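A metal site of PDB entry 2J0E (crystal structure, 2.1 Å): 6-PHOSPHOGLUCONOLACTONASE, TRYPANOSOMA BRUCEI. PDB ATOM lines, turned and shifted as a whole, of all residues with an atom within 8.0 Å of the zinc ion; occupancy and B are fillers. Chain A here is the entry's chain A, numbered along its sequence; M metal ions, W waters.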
ATOM      1  N   HIS A  56      -4.553  -4.943  -5.459  1.00  0.00           N
ATOM      2  CA  HIS A  56      -3.658  -4.987  -6.602  1.00  0.00           C
ATOM      3  C   HIS A  56      -3.044  -3.614  -6.895  1.00  0.00           C
ATOM      4  O   HIS A  56      -1.848  -3.505  -7.151  1.00  0.00           O
ATOM      5  CB  HIS A  56      -4.410  -5.501  -7.837  1.00  0.00           C
ATOM      6  CG  HIS A  56      -3.649  -5.370  -9.124  1.00  0.00           C
ATOM      7  ND1 HIS A  56      -3.553  -4.179  -9.819  1.00  0.00           N
ATOM      8  CD2 HIS A  56      -2.955  -6.281  -9.853  1.00  0.00           C
ATOM      9  CE1 HIS A  56      -2.850  -4.370 -10.921  1.00  0.00           C
ATOM     10  NE2 HIS A  56      -2.479  -5.637 -10.965  1.00  0.00           N
ATOM     11  N   ASP A  57      -3.857  -2.576  -6.851  1.00  0.00           N
ATOM     12  CA  ASP A  57      -3.391  -1.228  -7.160  1.00  0.00           C
ATOM     13  C   ASP A  57      -2.534  -0.529  -6.118  1.00  0.00           C
ATOM     14  O   ASP A  57      -1.631   0.221  -6.464  1.00  0.00           O
ATOM     15  CB  ASP A  57      -4.580  -0.334  -7.499  1.00  0.00           C
ATOM     16  CG  ASP A  57      -5.364  -0.842  -8.693  1.00  0.00           C
ATOM     17  OD1 ASP A  57      -4.849  -1.729  -9.399  1.00  0.00           O
ATOM     18  OD2 ASP A  57      -6.487  -0.337  -8.926  1.00  0.00           O
ATOM     19  N   LEU A  60       0.656  -4.155  -3.569  1.00  0.00           N
ATOM     20  CA  LEU A  60       1.439  -5.274  -4.075  1.00  0.00           C
ATOM     21  C   LEU A  60       2.782  -5.436  -3.384  1.00  0.00           C
ATOM     22  O   LEU A  60       3.314  -6.535  -3.323  1.00  0.00           O
ATOM     23  CB  LEU A  60       1.658  -5.141  -5.591  1.00  0.00           C
ATOM     24  CG  LEU A  60       0.481  -5.556  -6.484  1.00  0.00           C
ATOM     25  CD1 LEU A  60       0.847  -5.349  -7.946  1.00  0.00           C
ATOM     26  CD2 LEU A  60       0.147  -7.031  -6.233  1.00  0.00           C
ATOM     27  N   ARG A  64       3.099  -8.961  -2.856  1.00  0.00           N
ATOM     28  CA  ARG A  64       4.060  -9.553  -3.768  1.00  0.00           C
ATOM     29  C   ARG A  64       5.476  -9.594  -3.212  1.00  0.00           C
ATOM     30  O   ARG A  64       6.042 -10.668  -3.010  1.00  0.00           O
ATOM     31  CB  ARG A  64       4.044  -8.789  -5.092  1.00  0.00           C
ATOM     32  CG  ARG A  64       4.935  -9.341  -6.170  1.00  0.00           C
ATOM     33  CD  ARG A  64       4.753  -8.550  -7.443  1.00  0.00           C
ATOM     34  NE  ARG A  64       5.620  -9.033  -8.516  1.00  0.00           N
ATOM     35  CZ  ARG A  64       5.650  -8.506  -9.736  1.00  0.00           C
ATOM     36  NH1 ARG A  64       4.857  -7.492 -10.043  1.00  0.00           N
ATOM     37  NH2 ARG A  64       6.475  -9.017 -10.652  1.00  0.00           N
ATOM     38  N   ARG A  92      -7.664 -14.218 -10.329  1.00  0.00           N
ATOM     39  CA  ARG A  92      -6.381 -14.207 -11.015  1.00  0.00           C
ATOM     40  C   ARG A  92      -6.277 -12.938 -11.868  1.00  0.00           C
ATOM     41  O   ARG A  92      -5.280 -12.219 -11.815  1.00  0.00           O
ATOM     42  CB  ARG A  92      -6.235 -15.434 -11.903  1.00  0.00           C
ATOM     43  CG  ARG A  92      -4.917 -15.503 -12.671  1.00  0.00           C
ATOM     44  CD  ARG A  92      -4.940 -16.630 -13.694  1.00  0.00           C
ATOM     45  NE  ARG A  92      -6.125 -16.554 -14.561  1.00  0.00           N
ATOM     46  CZ  ARG A  92      -6.413 -15.522 -15.352  1.00  0.00           C
ATOM     47  NH1 ARG A  92      -5.601 -14.475 -15.417  1.00  0.00           N
ATOM     48  NH2 ARG A  92      -7.514 -15.549 -16.088  1.00  0.00           N
ATOM     49  N   GLU A  93      -7.336 -12.686 -12.626  1.00  0.00           N
ATOM     50  CA  GLU A  93      -7.431 -11.529 -13.511  1.00  0.00           C
ATOM     51  C   GLU A  93      -7.197 -10.200 -12.776  1.00  0.00           C
ATOM     52  O   GLU A  93      -6.383  -9.384 -13.194  1.00  0.00           O
ATOM     53  CB  GLU A  93      -8.811 -11.497 -14.166  1.00  0.00           C
ATOM     54  CG  GLU A  93      -8.816 -11.765 -15.667  1.00  0.00           C
ATOM     55  CD  GLU A  93     -10.179 -12.208 -16.182  1.00  0.00           C
ATOM     56  OE1 GLU A  93     -11.202 -11.823 -15.580  1.00  0.00           O
ATOM     57  OE2 GLU A  93     -10.222 -12.950 -17.191  1.00  0.00           O
ATOM     58  N   VAL A  94      -7.915 -10.016 -11.674  1.00  0.00           N
ATOM     59  CA  VAL A  94      -7.816  -8.780 -10.923  1.00  0.00           C
ATOM     60  C   VAL A  94      -6.646  -8.661  -9.958  1.00  0.00           C
ATOM     61  O   VAL A  94      -6.212  -7.548  -9.642  1.00  0.00           O
ATOM     62  CB  VAL A  94      -9.134  -8.518 -10.136  1.00  0.00           C
ATOM     63  CG1 VAL A  94      -9.415  -9.686  -9.200  1.00  0.00           C
ATOM     64  CG2 VAL A  94      -9.026  -7.253  -9.341  1.00  0.00           C
ATOM     65  N   LEU A  95      -6.109  -9.792  -9.489  1.00  0.00           N
ATOM     66  CA  LEU A  95      -5.022  -9.727  -8.515  1.00  0.00           C
ATOM     67  C   LEU A  95      -3.959 -10.822  -8.482  1.00  0.00           C
ATOM     68  O   LEU A  95      -2.763 -10.535  -8.519  1.00  0.00           O
ATOM     69  CB  LEU A  95      -5.642  -9.630  -7.110  1.00  0.00           C
ATOM     70  CG  LEU A  95      -4.691  -9.822  -5.926  1.00  0.00           C
ATOM     71  CD1 LEU A  95      -3.707  -8.644  -5.856  1.00  0.00           C
ATOM     72  CD2 LEU A  95      -5.497  -9.919  -4.628  1.00  0.00           C
ATOM     73  N   LEU A  96      -4.393 -12.072  -8.393  1.00  0.00           N
ATOM     74  CA  LEU A  96      -3.457 -13.183  -8.275  1.00  0.00           C
ATOM     75  C   LEU A  96      -2.373 -13.333  -9.340  1.00  0.00           C
ATOM     76  O   LEU A  96      -1.351 -13.983  -9.105  1.00  0.00           O
ATOM     77  CB  LEU A  96      -4.236 -14.496  -8.106  1.00  0.00           C
ATOM     78  CG  LEU A  96      -5.277 -14.467  -6.981  1.00  0.00           C
ATOM     79  CD1 LEU A  96      -5.887 -15.863  -6.784  1.00  0.00           C
ATOM     80  CD2 LEU A  96      -4.629 -14.008  -5.679  1.00  0.00           C
ATOM     81  N   HIS A  97      -2.566 -12.737 -10.515  1.00  0.00           N
ATOM     82  CA  HIS A  97      -1.560 -12.835 -11.567  1.00  0.00           C
ATOM     83  C   HIS A  97      -0.219 -12.232 -11.106  1.00  0.00           C
ATOM     84  O   HIS A  97       0.837 -12.592 -11.618  1.00  0.00           O
ATOM     85  CB  HIS A  97      -2.030 -12.152 -12.848  1.00  0.00           C
ATOM     86  CG  HIS A  97      -2.354 -10.697 -12.680  1.00  0.00           C
ATOM     87  ND1 HIS A  97      -3.628 -10.243 -12.420  1.00  0.00           N
ATOM     88  CD2 HIS A  97      -1.553  -9.603 -12.685  1.00  0.00           C
ATOM     89  CE1 HIS A  97      -3.593  -8.927 -12.281  1.00  0.00           C
ATOM     90  NE2 HIS A  97      -2.355  -8.520 -12.440  1.00  0.00           N
ATOM     91  N   ASP A  98      -0.283 -11.317 -10.130  1.00  0.00           N
ATOM     92  CA  ASP A  98       0.906 -10.645  -9.606  1.00  0.00           C
ATOM     93  C   ASP A  98       1.427 -11.285  -8.318  1.00  0.00           C
ATOM     94  O   ASP A  98       2.352 -10.759  -7.676  1.00  0.00           O
ATOM     95  CB  ASP A  98       0.591  -9.170  -9.340  1.00  0.00           C
ATOM     96  CG  ASP A  98       0.619  -8.337 -10.599  1.00  0.00           C
ATOM     97  OD1 ASP A  98      -0.067  -7.287 -10.655  1.00  0.00           O
ATOM     98  OD2 ASP A  98       1.336  -8.715 -11.545  1.00  0.00           O
ATOM     99  N   ILE A  99       0.844 -12.412  -7.931  1.00  0.00           N
ATOM    100  CA  ILE A  99       1.254 -13.098  -6.717  1.00  0.00           C
ATOM    101  C   ILE A  99       2.138 -14.302  -7.001  1.00  0.00           C
ATOM    102  O   ILE A  99       1.838 -15.104  -7.875  1.00  0.00           O
ATOM    103  CB  ILE A  99       0.017 -13.565  -5.916  1.00  0.00           C
ATOM    104  CG1 ILE A  99      -0.901 -12.380  -5.614  1.00  0.00           C
ATOM    105  CG2 ILE A  99       0.470 -14.252  -4.620  1.00  0.00           C
ATOM    106  CD1 ILE A  99      -0.240 -11.296  -4.763  1.00  0.00           C
HETATM  107 ZN    ZN M   1      -1.131  -6.535 -12.243  1.00  0.00          ZN
HETATM  108  O   HOH W   1       0.488  -4.712 -11.652  1.00  0.00           O
HETATM  109  O   HOH W   2      -2.104  -5.718 -14.047  1.00  0.00           O
HETATM  110  O   HOH W   3       0.565  -7.238 -13.662  1.00  0.00           O
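Within 4 Å of the zinc ion: His 56, His 97 and Asp 98.
The nearest printed residue that does not touch the zinc ion is Leu 60 (4.9 Å).
A ring nitrogen (ND1) of His 97 is in hydrogen-bond range of the backbone carbonyl oxygen (O) of Arg 92, at 2.6 Å.
A ring nitrogen (ND1) of His 97 lies close to the backbone carbonyl oxygen of Glu 93.
The side-chain carboxylate (OD1) of Asp 57 lies within hydrogen-bond range of a ring nitrogen (ND1) of His 56, at 2.8 Å.
The zinc ion is bound by the side-chain carboxylate of Asp 98 (2.1 Å), a ring nitrogen (NE2) of His 56 (2.1 Å), water W2 (2.2 Å), water W3 (2.3 Å), a ring nitrogen (NE2) of His 97 (2.3 Å) and water W1 (2.5 Å).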
